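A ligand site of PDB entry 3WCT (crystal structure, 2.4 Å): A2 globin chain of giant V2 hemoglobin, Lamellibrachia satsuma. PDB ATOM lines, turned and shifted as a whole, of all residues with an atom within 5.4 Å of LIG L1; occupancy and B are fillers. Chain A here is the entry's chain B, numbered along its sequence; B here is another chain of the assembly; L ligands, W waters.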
ATOM      1  N   TRP A  33      -8.604  14.278 -19.780  1.00  0.00           N
ATOM      2  CA  TRP A  33      -9.836  14.916 -20.224  1.00  0.00           C
ATOM      3  C   TRP A  33     -10.210  14.667 -21.674  1.00  0.00           C
ATOM      4  O   TRP A  33     -11.381  14.822 -22.042  1.00  0.00           O
ATOM      5  CB  TRP A  33      -9.808  16.405 -19.903  1.00  0.00           C
ATOM      6  CG  TRP A  33     -10.026  16.630 -18.446  1.00  0.00           C
ATOM      7  CD1 TRP A  33      -9.063  16.707 -17.465  1.00  0.00           C
ATOM      8  CD2 TRP A  33     -11.289  16.663 -17.771  1.00  0.00           C
ATOM      9  NE1 TRP A  33      -9.659  16.778 -16.224  1.00  0.00           N
ATOM     10  CE2 TRP A  33     -11.024  16.754 -16.385  1.00  0.00           C
ATOM     11  CE3 TRP A  33     -12.624  16.621 -18.202  1.00  0.00           C
ATOM     12  CZ2 TRP A  33     -12.034  16.802 -15.426  1.00  0.00           C
ATOM     13  CZ3 TRP A  33     -13.633  16.666 -17.253  1.00  0.00           C
ATOM     14  CH2 TRP A  33     -13.338  16.757 -15.876  1.00  0.00           C
ATOM     15  N   ALA A  43     -21.191  15.303 -21.202  1.00  0.00           N
ATOM     16  CA  ALA A  43     -20.717  15.991 -20.014  1.00  0.00           C
ATOM     17  C   ALA A  43     -20.032  17.347 -20.193  1.00  0.00           C
ATOM     18  O   ALA A  43     -20.040  18.151 -19.271  1.00  0.00           O
ATOM     19  CB  ALA A  43     -19.799  15.070 -19.236  1.00  0.00           C
ATOM     20  N   MET A  46     -21.345  20.801 -18.875  1.00  0.00           N
ATOM     21  CA  MET A  46     -21.202  21.284 -17.503  1.00  0.00           C
ATOM     22  C   MET A  46     -19.973  22.189 -17.322  1.00  0.00           C
ATOM     23  O   MET A  46     -19.836  22.864 -16.306  1.00  0.00           O
ATOM     24  CB  MET A  46     -21.073  20.103 -16.543  1.00  0.00           C
ATOM     25  CG  MET A  46     -22.354  19.304 -16.392  1.00  0.00           C
ATOM     26  SD  MET A  46     -22.101  17.862 -15.363  1.00  0.00           S
ATOM     27  CE  MET A  46     -21.393  18.635 -13.899  1.00  0.00           C
ATOM     28  N   PHE A  47     -19.103  22.212 -18.330  1.00  0.00           N
ATOM     29  CA  PHE A  47     -17.886  22.999 -18.276  1.00  0.00           C
ATOM     30  C   PHE A  47     -17.918  24.266 -19.133  1.00  0.00           C
ATOM     31  O   PHE A  47     -16.876  24.724 -19.599  1.00  0.00           O
ATOM     32  CB  PHE A  47     -16.702  22.126 -18.670  1.00  0.00           C
ATOM     33  CG  PHE A  47     -16.491  20.951 -17.771  1.00  0.00           C
ATOM     34  CD1 PHE A  47     -15.782  21.082 -16.583  1.00  0.00           C
ATOM     35  CD2 PHE A  47     -17.059  19.723 -18.065  1.00  0.00           C
ATOM     36  CE1 PHE A  47     -15.635  20.019 -15.711  1.00  0.00           C
ATOM     37  CE2 PHE A  47     -16.920  18.646 -17.199  1.00  0.00           C
ATOM     38  CZ  PHE A  47     -16.214  18.795 -16.017  1.00  0.00           C
ATOM     39  N   ARG A  49     -18.183  27.378 -18.386  1.00  0.00           N
ATOM     40  CA  ARG A  49     -17.350  28.459 -17.863  1.00  0.00           C
ATOM     41  C   ARG A  49     -15.848  28.277 -18.063  1.00  0.00           C
ATOM     42  O   ARG A  49     -15.100  29.261 -18.026  1.00  0.00           O
ATOM     43  CB  ARG A  49     -17.639  28.680 -16.367  1.00  0.00           C
ATOM     44  CG  ARG A  49     -17.164  30.029 -15.827  1.00  0.00           C
ATOM     45  CD  ARG A  49     -17.313  30.096 -14.324  1.00  0.00           C
ATOM     46  NE  ARG A  49     -16.401  29.161 -13.659  1.00  0.00           N
ATOM     47  CZ  ARG A  49     -15.089  29.370 -13.532  1.00  0.00           C
ATOM     48  NH1 ARG A  49     -14.536  30.480 -14.012  1.00  0.00           N
ATOM     49  NH2 ARG A  49     -14.328  28.449 -12.949  1.00  0.00           N
ATOM     50  N   VAL A  50     -15.398  27.040 -18.252  1.00  0.00           N
ATOM     51  CA  VAL A  50     -13.970  26.802 -18.436  1.00  0.00           C
ATOM     52  C   VAL A  50     -13.623  26.276 -19.818  1.00  0.00           C
ATOM     53  O   VAL A  50     -12.654  25.537 -20.002  1.00  0.00           O
ATOM     54  CB  VAL A  50     -13.422  25.859 -17.332  1.00  0.00           C
ATOM     55  CG1 VAL A  50     -13.792  26.410 -15.962  1.00  0.00           C
ATOM     56  CG2 VAL A  50     -13.950  24.458 -17.501  1.00  0.00           C
ATOM     57  N   HIS A  63      -8.340  24.588 -15.490  1.00  0.00           N
ATOM     58  CA  HIS A  63      -9.307  23.744 -14.791  1.00  0.00           C
ATOM     59  C   HIS A  63      -8.703  22.332 -14.598  1.00  0.00           C
ATOM     60  O   HIS A  63      -8.722  21.793 -13.482  1.00  0.00           O
ATOM     61  CB  HIS A  63     -10.625  23.644 -15.587  1.00  0.00           C
ATOM     62  CG  HIS A  63     -11.521  22.537 -15.134  1.00  0.00           C
ATOM     63  ND1 HIS A  63     -12.257  22.613 -13.971  1.00  0.00           N
ATOM     64  CD2 HIS A  63     -11.728  21.292 -15.629  1.00  0.00           C
ATOM     65  CE1 HIS A  63     -12.878  21.459 -13.769  1.00  0.00           C
ATOM     66  NE2 HIS A  63     -12.573  20.637 -14.769  1.00  0.00           N
ATOM     67  N   ARG A  66      -6.452  22.399 -11.874  1.00  0.00           N
ATOM     68  CA  ARG A  66      -7.127  22.364 -10.577  1.00  0.00           C
ATOM     69  C   ARG A  66      -7.590  20.972 -10.205  1.00  0.00           C
ATOM     70  O   ARG A  66      -7.358  20.519  -9.082  1.00  0.00           O
ATOM     71  CB  ARG A  66      -8.322  23.316 -10.549  1.00  0.00           C
ATOM     72  CG  ARG A  66      -7.928  24.783 -10.579  1.00  0.00           C
ATOM     73  CD  ARG A  66      -9.116  25.707 -10.248  1.00  0.00           C
ATOM     74  NE  ARG A  66     -10.130  25.724 -11.303  1.00  0.00           N
ATOM     75  CZ  ARG A  66     -10.040  26.409 -12.428  1.00  0.00           C
ATOM     76  NH1 ARG A  66     -11.028  26.353 -13.322  1.00  0.00           N
ATOM     77  NH2 ARG A  66      -8.982  27.169 -12.688  1.00  0.00           N
ATOM     78  N   VAL A  67      -8.242  20.285 -11.148  1.00  0.00           N
ATOM     79  CA  VAL A  67      -8.757  18.929 -10.913  1.00  0.00           C
ATOM     80  C   VAL A  67      -7.664  17.964 -10.459  1.00  0.00           C
ATOM     81  O   VAL A  67      -7.830  17.260  -9.462  1.00  0.00           O
ATOM     82  CB  VAL A  67      -9.393  18.336 -12.194  1.00  0.00           C
ATOM     83  CG1 VAL A  67      -9.782  16.869 -11.949  1.00  0.00           C
ATOM     84  CG2 VAL A  67     -10.588  19.148 -12.596  1.00  0.00           C
ATOM     85  N   GLY A  70      -6.607  18.417  -7.226  1.00  0.00           N
ATOM     86  CA  GLY A  70      -7.571  17.883  -6.272  1.00  0.00           C
ATOM     87  C   GLY A  70      -7.303  16.405  -6.035  1.00  0.00           C
ATOM     88  O   GLY A  70      -7.320  15.927  -4.901  1.00  0.00           O
ATOM     89  N   LEU A  71      -7.049  15.687  -7.112  1.00  0.00           N
ATOM     90  CA  LEU A  71      -6.745  14.266  -7.014  1.00  0.00           C
ATOM     91  C   LEU A  71      -5.469  14.070  -6.213  1.00  0.00           C
ATOM     92  O   LEU A  71      -5.364  13.114  -5.441  1.00  0.00           O
ATOM     93  CB  LEU A  71      -6.541  13.676  -8.404  1.00  0.00           C
ATOM     94  CG  LEU A  71      -7.727  12.998  -9.059  1.00  0.00           C
ATOM     95  CD1 LEU A  71      -7.378  12.626 -10.490  1.00  0.00           C
ATOM     96  CD2 LEU A  71      -8.092  11.773  -8.249  1.00  0.00           C
ATOM     97  N   CYS A  74      -6.018  14.284  -2.450  1.00  0.00           N
ATOM     98  CA  CYS A  74      -6.650  13.078  -1.970  1.00  0.00           C
ATOM     99  C   CYS A  74      -5.670  11.900  -1.927  1.00  0.00           C
ATOM    100  O   CYS A  74      -5.656  11.142  -0.959  1.00  0.00           O
ATOM    101  CB  CYS A  74      -7.862  12.722  -2.840  1.00  0.00           C
ATOM    102  SG  CYS A  74      -9.111  14.034  -2.926  1.00  0.00           S
ATOM    103  N   LEU A  91     -14.310  19.010  -1.462  1.00  0.00           N
ATOM    104  CA  LEU A  91     -14.571  18.745  -2.876  1.00  0.00           C
ATOM    105  C   LEU A  91     -16.069  18.519  -3.097  1.00  0.00           C
ATOM    106  O   LEU A  91     -16.619  18.912  -4.113  1.00  0.00           O
ATOM    107  CB  LEU A  91     -13.792  17.506  -3.330  1.00  0.00           C
ATOM    108  CG  LEU A  91     -12.304  17.684  -3.629  1.00  0.00           C
ATOM    109  CD1 LEU A  91     -11.649  16.324  -3.754  1.00  0.00           C
ATOM    110  CD2 LEU A  91     -12.133  18.480  -4.910  1.00  0.00           C
ATOM    111  N   GLN A  94     -17.785  21.688  -3.497  1.00  0.00           N
ATOM    112  CA  GLN A  94     -17.399  22.377  -4.730  1.00  0.00           C
ATOM    113  C   GLN A  94     -18.152  21.812  -5.934  1.00  0.00           C
ATOM    114  O   GLN A  94     -18.173  22.419  -7.004  1.00  0.00           O
ATOM    115  CB  GLN A  94     -15.889  22.290  -4.966  1.00  0.00           C
ATOM    116  CG  GLN A  94     -15.047  23.054  -3.941  1.00  0.00           C
ATOM    117  CD  GLN A  94     -13.559  22.910  -4.178  1.00  0.00           C
ATOM    118  OE1 GLN A  94     -13.037  21.791  -4.258  1.00  0.00           O
ATOM    119  NE2 GLN A  94     -12.856  24.035  -4.287  1.00  0.00           N
ATOM    120  N   HIS A  95     -18.770  20.641  -5.747  1.00  0.00           N
ATOM    121  CA  HIS A  95     -19.542  19.965  -6.791  1.00  0.00           C
ATOM    122  C   HIS A  95     -21.035  19.815  -6.448  1.00  0.00           C
ATOM    123  O   HIS A  95     -21.805  19.315  -7.270  1.00  0.00           O
ATOM    124  CB  HIS A  95     -18.989  18.567  -7.059  1.00  0.00           C
ATOM    125  CG  HIS A  95     -17.618  18.542  -7.665  1.00  0.00           C
ATOM    126  ND1 HIS A  95     -16.484  18.906  -6.966  1.00  0.00           N
ATOM    127  CD2 HIS A  95     -17.208  18.198  -8.910  1.00  0.00           C
ATOM    128  CE1 HIS A  95     -15.438  18.781  -7.752  1.00  0.00           C
ATOM    129  NE2 HIS A  95     -15.845  18.351  -8.939  1.00  0.00           N
ATOM    130  N   ARG A  98     -23.904  21.259  -8.899  1.00  0.00           N
ATOM    131  CA  ARG A  98     -23.623  21.007 -10.308  1.00  0.00           C
ATOM    132  C   ARG A  98     -24.238  19.728 -10.875  1.00  0.00           C
ATOM    133  O   ARG A  98     -24.109  19.446 -12.069  1.00  0.00           O
ATOM    134  CB  ARG A  98     -22.115  21.019 -10.540  1.00  0.00           C
ATOM    135  CG  ARG A  98     -21.446  22.269  -9.979  1.00  0.00           C
ATOM    136  CD  ARG A  98     -19.931  22.196 -10.048  1.00  0.00           C
ATOM    137  NE  ARG A  98     -19.307  23.405  -9.495  1.00  0.00           N
ATOM    138  CZ  ARG A  98     -19.369  24.612 -10.062  1.00  0.00           C
ATOM    139  NH1 ARG A  98     -18.763  25.645  -9.484  1.00  0.00           N
ATOM    140  NH2 ARG A  98     -20.008  24.787 -11.214  1.00  0.00           N
ATOM    141  N   VAL A 100     -23.588  16.249 -10.576  1.00  0.00           N
ATOM    142  CA  VAL A 100     -22.716  15.260 -11.218  1.00  0.00           C
ATOM    143  C   VAL A 100     -23.292  13.887 -10.873  1.00  0.00           C
ATOM    144  O   VAL A 100     -23.599  13.613  -9.711  1.00  0.00           O
ATOM    145  CB  VAL A 100     -21.246  15.334 -10.692  1.00  0.00           C
ATOM    146  CG1 VAL A 100     -20.385  14.291 -11.410  1.00  0.00           C
ATOM    147  CG2 VAL A 100     -20.676  16.727 -10.905  1.00  0.00           C
ATOM    148  N   GLN A 104     -20.888   9.747 -14.218  1.00  0.00           N
ATOM    149  CA  GLN A 104     -19.831  10.629 -14.688  1.00  0.00           C
ATOM    150  C   GLN A 104     -18.607  10.508 -13.791  1.00  0.00           C
ATOM    151  O   GLN A 104     -17.477  10.669 -14.241  1.00  0.00           O
ATOM    152  CB  GLN A 104     -20.332  12.082 -14.728  1.00  0.00           C
ATOM    153  CG  GLN A 104     -21.515  12.284 -15.675  1.00  0.00           C
ATOM    154  CD  GLN A 104     -22.035  13.715 -15.686  1.00  0.00           C
ATOM    155  OE1 GLN A 104     -22.424  14.250 -14.645  1.00  0.00           O
ATOM    156  NE2 GLN A 104     -22.045  14.337 -16.858  1.00  0.00           N
ATOM    157  N   TYR A 105     -18.826  10.231 -12.503  1.00  0.00           N
ATOM    158  CA  TYR A 105     -17.711  10.085 -11.584  1.00  0.00           C
ATOM    159  C   TYR A 105     -16.906   8.870 -12.012  1.00  0.00           C
ATOM    160  O   TYR A 105     -15.681   8.936 -12.105  1.00  0.00           O
ATOM    161  CB  TYR A 105     -18.210   9.911 -10.142  1.00  0.00           C
ATOM    162  CG  TYR A 105     -18.401  11.231  -9.448  1.00  0.00           C
ATOM    163  CD1 TYR A 105     -17.316  12.071  -9.221  1.00  0.00           C
ATOM    164  CD2 TYR A 105     -19.669  11.674  -9.075  1.00  0.00           C
ATOM    165  CE1 TYR A 105     -17.485  13.321  -8.627  1.00  0.00           C
ATOM    166  CE2 TYR A 105     -19.849  12.931  -8.485  1.00  0.00           C
ATOM    167  CZ  TYR A 105     -18.751  13.747  -8.268  1.00  0.00           C
ATOM    168  OH  TYR A 105     -18.910  15.011  -7.722  1.00  0.00           O
ATOM    169  N   VAL A 108     -14.691   9.610 -15.171  1.00  0.00           N
ATOM    170  CA  VAL A 108     -13.455  10.273 -14.808  1.00  0.00           C
ATOM    171  C   VAL A 108     -12.489   9.305 -14.137  1.00  0.00           C
ATOM    172  O   VAL A 108     -11.278   9.418 -14.324  1.00  0.00           O
ATOM    173  CB  VAL A 108     -13.768  11.478 -13.906  1.00  0.00           C
ATOM    174  CG1 VAL A 108     -12.483  12.122 -13.392  1.00  0.00           C
ATOM    175  CG2 VAL A 108     -14.578  12.511 -14.710  1.00  0.00           C
ATOM    176  N   VAL A 112      -8.888   8.650 -15.464  1.00  0.00           N
ATOM    177  CA  VAL A 112      -7.720   8.807 -14.616  1.00  0.00           C
ATOM    178  C   VAL A 112      -6.811   7.577 -14.654  1.00  0.00           C
ATOM    179  O   VAL A 112      -5.594   7.695 -14.725  1.00  0.00           O
ATOM    180  CB  VAL A 112      -8.108   9.090 -13.152  1.00  0.00           C
ATOM    181  CG1 VAL A 112      -6.917   8.832 -12.237  1.00  0.00           C
ATOM    182  CG2 VAL A 112      -8.565  10.556 -13.011  1.00  0.00           C
ATOM    183  N   ILE A 137     -12.418   7.659  -3.139  1.00  0.00           N
ATOM    184  CA  ILE A 137     -12.327   9.093  -3.352  1.00  0.00           C
ATOM    185  C   ILE A 137     -13.599   9.748  -3.902  1.00  0.00           C
ATOM    186  O   ILE A 137     -14.085  10.722  -3.332  1.00  0.00           O
ATOM    187  CB  ILE A 137     -11.118   9.432  -4.243  1.00  0.00           C
ATOM    188  CG1 ILE A 137      -9.824   9.111  -3.488  1.00  0.00           C
ATOM    189  CG2 ILE A 137     -11.168  10.905  -4.665  1.00  0.00           C
ATOM    190  CD1 ILE A 137      -8.561   9.034  -4.352  1.00  0.00           C
ATOM    191  N   THR A 138     -14.129   9.231  -5.001  1.00  0.00           N
ATOM    192  CA  THR A 138     -15.327   9.797  -5.607  1.00  0.00           C
ATOM    193  C   THR A 138     -16.533   9.583  -4.701  1.00  0.00           C
ATOM    194  O   THR A 138     -17.380  10.465  -4.521  1.00  0.00           O
ATOM    195  CB  THR A 138     -15.632   9.159  -6.964  1.00  0.00           C
ATOM    196  OG1 THR A 138     -15.858   7.764  -6.777  1.00  0.00           O
ATOM    197  CG2 THR A 138     -14.463   9.353  -7.908  1.00  0.00           C
ATOM    198  N   ILE A 141     -16.648  12.256  -2.475  1.00  0.00           N
ATOM    199  CA  ILE A 141     -16.943  13.549  -3.083  1.00  0.00           C
ATOM    200  C   ILE A 141     -18.442  13.649  -3.357  1.00  0.00           C
ATOM    201  O   ILE A 141     -18.976  14.753  -3.499  1.00  0.00           O
ATOM    202  CB  ILE A 141     -16.158  13.751  -4.405  1.00  0.00           C
ATOM    203  CG1 ILE A 141     -14.657  13.715  -4.135  1.00  0.00           C
ATOM    204  CG2 ILE A 141     -16.517  15.078  -5.042  1.00  0.00           C
ATOM    205  CD1 ILE A 141     -13.805  13.847  -5.381  1.00  0.00           C
ATOM    206  N   HIS B  94      -8.521  32.740 -11.117  1.00  0.00           N
ATOM    207  CA  HIS B  94      -9.408  31.888 -10.355  1.00  0.00           C
ATOM    208  C   HIS B  94      -9.087  31.996  -8.864  1.00  0.00           C
ATOM    209  O   HIS B  94      -9.980  32.097  -8.025  1.00  0.00           O
ATOM    210  CB  HIS B  94      -9.258  30.443 -10.809  1.00  0.00           C
ATOM    211  CG  HIS B  94     -10.240  29.504 -10.181  1.00  0.00           C
ATOM    212  ND1 HIS B  94     -11.488  29.278 -10.717  1.00  0.00           N
ATOM    213  CD2 HIS B  94     -10.158  28.730  -9.083  1.00  0.00           C
ATOM    214  CE1 HIS B  94     -12.129  28.397  -9.967  1.00  0.00           C
ATOM    215  NE2 HIS B  94     -11.342  28.047  -8.971  1.00  0.00           N
ATOM    216  N   GLN B  98     -11.154  33.646  -5.579  1.00  0.00           N
ATOM    217  CA  GLN B  98     -11.344  32.850  -4.375  1.00  0.00           C
ATOM    218  C   GLN B  98     -10.909  33.598  -3.106  1.00  0.00           C
ATOM    219  O   GLN B  98     -11.214  33.161  -1.999  1.00  0.00           O
ATOM    220  CB  GLN B  98     -10.582  31.521  -4.483  1.00  0.00           C
ATOM    221  CG  GLN B  98     -11.154  30.548  -5.513  1.00  0.00           C
ATOM    222  CD  GLN B  98     -10.377  29.244  -5.564  1.00  0.00           C
ATOM    223  OE1 GLN B  98      -9.153  29.250  -5.698  1.00  0.00           O
ATOM    224  NE2 GLN B  98     -11.080  28.123  -5.468  1.00  0.00           N
HETATM  225  C1  LIG L   1     -14.560  21.728 -10.579  1.00  0.00           C
HETATM  226  C2  LIG L   1     -11.914  18.251  -8.693  1.00  0.00           C
HETATM  227  C3  LIG L   1     -14.774  14.911 -10.713  1.00  0.00           C
HETATM  228  C4  LIG L   1     -17.324  18.454 -12.737  1.00  0.00           C
HETATM  229  C5  LIG L   1     -13.565  21.078  -9.880  1.00  0.00           C
HETATM  230  C6  LIG L   1     -12.550  21.741  -9.157  1.00  0.00           C
HETATM  231  C7  LIG L   1     -11.789  20.752  -8.633  1.00  0.00           C
HETATM  232  C8  LIG L   1     -12.347  19.466  -9.021  1.00  0.00           C
HETATM  233  C9  LIG L   1     -10.540  20.903  -7.745  1.00  0.00           C
HETATM  234  C10 LIG L   1     -12.348  23.248  -9.002  1.00  0.00           C
HETATM  235  C11 LIG L   1     -13.248  23.816  -7.916  1.00  0.00           C
HETATM  236  C12 LIG L   1     -13.159  25.330  -7.686  1.00  0.00           C
HETATM  237  O1  LIG L   1     -12.046  25.880  -7.461  1.00  0.00           O
HETATM  238  O2  LIG L   1     -14.189  25.961  -7.724  1.00  0.00           O
HETATM  239  C13 LIG L   1     -12.478  17.001  -9.041  1.00  0.00           C
HETATM  240  C14 LIG L   1     -11.950  15.729  -8.586  1.00  0.00           C
HETATM  241  C15 LIG L   1     -12.815  14.745  -9.181  1.00  0.00           C
HETATM  242  C16 LIG L   1     -13.759  15.484  -9.945  1.00  0.00           C
HETATM  243  C17 LIG L   1     -10.785  15.520  -7.702  1.00  0.00           C
HETATM  244  C18 LIG L   1     -12.654  13.322  -8.964  1.00  0.00           C
HETATM  245  C19 LIG L   1     -12.345  12.454  -9.892  1.00  0.00           C
HETATM  246  C20 LIG L   1     -15.694  15.613 -11.470  1.00  0.00           C
HETATM  247  C21 LIG L   1     -16.714  14.934 -12.284  1.00  0.00           C
HETATM  248  C22 LIG L   1     -17.443  15.938 -12.941  1.00  0.00           C
HETATM  249  C23 LIG L   1     -16.849  17.226 -12.400  1.00  0.00           C
HETATM  250  C24 LIG L   1     -16.906  13.420 -12.403  1.00  0.00           C
HETATM  251  C25 LIG L   1     -18.438  15.778 -13.849  1.00  0.00           C
HETATM  252  C26 LIG L   1     -18.578  15.317 -15.058  1.00  0.00           C
HETATM  253  C27 LIG L   1     -16.809  19.671 -12.293  1.00  0.00           C
HETATM  254  C28 LIG L   1     -17.387  21.008 -12.680  1.00  0.00           C
HETATM  255  C29 LIG L   1     -16.585  21.927 -12.064  1.00  0.00           C
HETATM  256  C30 LIG L   1     -15.558  21.172 -11.310  1.00  0.00           C
HETATM  257  C31 LIG L   1     -18.588  21.191 -13.589  1.00  0.00           C
HETATM  258  C32 LIG L   1     -16.722  23.443 -12.112  1.00  0.00           C
HETATM  259  C33 LIG L   1     -15.891  24.093 -13.197  1.00  0.00           C
HETATM  260  C34 LIG L   1     -15.955  25.573 -13.139  1.00  0.00           C
HETATM  261  O3  LIG L   1     -15.199  26.197 -12.356  1.00  0.00           O
HETATM  262  O4  LIG L   1     -16.743  26.191 -13.874  1.00  0.00           O
HETATM  263  N1  LIG L   1     -13.454  19.678  -9.805  1.00  0.00           N
HETATM  264  N2  LIG L   1     -13.553  16.892  -9.825  1.00  0.00           N
HETATM  265  N3  LIG L   1     -15.811  16.991 -11.569  1.00  0.00           N
HETATM  266  N4  LIG L   1     -15.750  19.825 -11.474  1.00  0.00           N
HETATM  267 FE1  LIG L   1     -14.649  18.342 -10.664  1.00  0.00          FE
HETATM  268  O1  LG2 L   2     -13.645  18.364 -12.147  1.00  0.00           O
HETATM  269  O2  LG2 L   2     -13.788  18.465 -13.361  1.00  0.00           O
HETATM  270  C1  LG3 L   3      -8.434  30.102   0.778  1.00  0.00           C
HETATM  271  C2  LG3 L   3      -4.362  29.681  -1.617  1.00  0.00           C
HETATM  272  C3  LG3 L   3      -2.556  33.555   0.618  1.00  0.00           C
HETATM  273  C4  LG3 L   3      -6.779  34.071   2.889  1.00  0.00           C
HETATM  274  C5  LG3 L   3      -7.484  29.646  -0.100  1.00  0.00           C
HETATM  275  C6  LG3 L   3      -7.656  28.500  -0.901  1.00  0.00           C
HETATM  276  C7  LG3 L   3      -6.504  28.390  -1.598  1.00  0.00           C
HETATM  277  C8  LG3 L   3      -5.605  29.459  -1.206  1.00  0.00           C
HETATM  278  C9  LG3 L   3      -6.144  27.307  -2.642  1.00  0.00           C
HETATM  279  C10 LG3 L   3      -8.854  27.562  -0.958  1.00  0.00           C
HETATM  280  C11 LG3 L   3      -9.843  27.927  -2.019  1.00  0.00           C
HETATM  281  C12 LG3 L   3     -11.049  26.986  -2.109  1.00  0.00           C
HETATM  282  O1  LG3 L   3     -10.872  25.747  -2.275  1.00  0.00           O
HETATM  283  O2  LG3 L   3     -12.142  27.463  -2.025  1.00  0.00           O
HETATM  284  C13 LG3 L   3      -3.456  30.692  -1.212  1.00  0.00           C
HETATM  285  C14 LG3 L   3      -2.097  30.809  -1.703  1.00  0.00           C
HETATM  286  C15 LG3 L   3      -1.569  31.963  -1.017  1.00  0.00           C
HETATM  287  C16 LG3 L   3      -2.630  32.433  -0.207  1.00  0.00           C
HETATM  288  C17 LG3 L   3      -1.420  29.922  -2.680  1.00  0.00           C
HETATM  289  C18 LG3 L   3      -0.206  32.448  -1.189  1.00  0.00           C
HETATM  290  C19 LG3 L   3       0.157  33.325  -2.109  1.00  0.00           C
HETATM  291  C20 LG3 L   3      -3.590  34.048   1.421  1.00  0.00           C
HETATM  292  C21 LG3 L   3      -3.437  35.263   2.237  1.00  0.00           C
HETATM  293  C22 LG3 L   3      -4.662  35.464   2.914  1.00  0.00           C
HETATM  294  C23 LG3 L   3      -5.513  34.281   2.441  1.00  0.00           C
HETATM  295  C24 LG3 L   3      -2.191  36.128   2.316  1.00  0.00           C
HETATM  296  C25 LG3 L   3      -4.988  36.476   3.773  1.00  0.00           C
HETATM  297  C26 LG3 L   3      -4.662  36.920   4.938  1.00  0.00           C
HETATM  298  C27 LG3 L   3      -7.600  33.014   2.531  1.00  0.00           C
HETATM  299  C28 LG3 L   3      -8.967  32.783   3.119  1.00  0.00           C
HETATM  300  C29 LG3 L   3      -9.406  31.629   2.515  1.00  0.00           C
HETATM  301  C30 LG3 L   3      -8.346  31.197   1.583  1.00  0.00           C
HETATM  302  C31 LG3 L   3      -9.636  33.684   4.156  1.00  0.00           C
HETATM  303  C32 LG3 L   3     -10.709  30.906   2.753  1.00  0.00           C
HETATM  304  C33 LG3 L   3     -10.518  29.786   3.737  1.00  0.00           C
HETATM  305  C34 LG3 L   3     -11.704  28.949   3.899  1.00  0.00           C
HETATM  306  O3  LG3 L   3     -12.550  29.228   4.791  1.00  0.00           O
HETATM  307  O4  LG3 L   3     -11.848  27.960   3.157  1.00  0.00           O
HETATM  308  N1  LG3 L   3      -6.237  30.253  -0.285  1.00  0.00           N
HETATM  309  N2  LG3 L   3      -3.804  31.635  -0.328  1.00  0.00           N
HETATM  310  N3  LG3 L   3      -4.864  33.504   1.558  1.00  0.00           N
HETATM  311  N4  LG3 L   3      -7.278  32.044   1.644  1.00  0.00           N
HETATM  312 FE1  LG3 L   3      -5.557  31.887   0.633  1.00  0.00          FE
HETATM  313  O   HOH W   1      -9.661  24.681  -6.654  1.00  0.00           O
HETATM  314  O   HOH W   2     -17.091  24.823  -6.800  1.00  0.00           O
HETATM  315  O   HOH W   3     -12.637  24.858 -12.190  1.00  0.00           O
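FE1 of LIG L1 is bound by NE2 of His 95, at 2.1 Å. The guanidinium group (NH2) of Arg 49 lies within salt-bridge range of an oxygen (O3) of LIG L1 (2.5 Å). NE2 of His 94 of chain B lies within hydrogen-bond range of O1 of LIG L1 (2.7 Å). O1 of LIG L1 sits at hydrogen-bond distance from NE2 of Gln 98 of chain B (3.2 Å). NE2 of His 63 sits at hydrogen-bond distance from O2 of LG2 L2. The side-chain amide nitrogen (NE2) of Gln 94 of chain A sits at hydrogen-bond distance from an oxygen (O1) of LG3 L3 (3.3 Å).
O of Met 46 touches C31 of LIG L1 (3.4 Å). Phe 47 touches LIG L1 (CZ to C4, 3.5 Å). Val 50 touches LIG L1 (CG1 to O4, 3.6 Å). His 63 touches LIG L1 (CE1 to C1, 3.6 Å). O of Arg 66 touches C9 of LIG L1, at 3.5 Å. Val 67 touches LIG L1 (O to C17, 3.9 Å). C of Gly 70 touches C17 of LIG L1, 3.96 Å away. Leu 71 touches LIG L1. Leu 91 touches LIG L1. Gln 94 of chain A touches LIG L1 (NE2 to C12, 3.6 Å). Arg 98 of chain A touches LIG L1. Val 100 touches LIG L1. Gln 104 touches LIG L1 (O to C24, 3.4 Å). CD1 of Tyr 105 touches C24 of LIG L1 (3.5 Å). Val 108 touches LIG L1. Ile 141 touches LIG L1. Hydrophobic or aromatic side chains within 4 Å of LIG L1: Met 46, Phe 47, Val 50, His 63, Val 67, Leu 91, His 95, Val 100, Tyr 105, Val 108, Ile 141 and His 94 of chain B. 20 residues have an atom within 4 Å of LIG L1: Met 46, Phe 47, Arg 49, Val 50, His 63, Arg 66, Val 67, Gly 70, Leu 71, Leu 91, Gln 94 of chain A, His 95, Arg 98 of chain A, Val 100, Gln 104, Tyr 105, Val 108, Ile 141, His 94 of chain B and Gln 98 of chain B. The nearest printed residue that does not touch LIG L1 is Thr 138 (4.2 Å).
A ring nitrogen (ND1) of His 95 lies within hydrogen-bond range of the backbone carbonyl oxygen (O) of Leu 91 (2.9 Å). The side-chain amide oxygen (OE1) of Gln 104 lies close to the side-chain sulfur (SD) of Met 46 (3.7 Å). The guanidinium group (NE) of Arg 98 of chain A sits at hydrogen-bond distance from the backbone carbonyl oxygen (O) of Gln 94 of chain A. O of Gly 70 sits at hydrogen-bond distance from SG of Cys 74 (3.3 Å).
An iron atom (FE1) of LIG L1 is bound by an oxygen (O1) of LG2 L2, 1.8 Å away.
Water W3 lies within hydrogen-bond range of the guanidinium group of Arg 66 (2.5 Å), a ring nitrogen (ND1) of His 63 (2.9 Å) and an oxygen (O3) of LIG L1 (2.9 Å). Water W2 lies within hydrogen-bond range of O of Gln 94 of chain A (2.6 Å), O2 of LIG L1 (3.3 Å) and NH1 of Arg 98 of chain A (3.3 Å).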
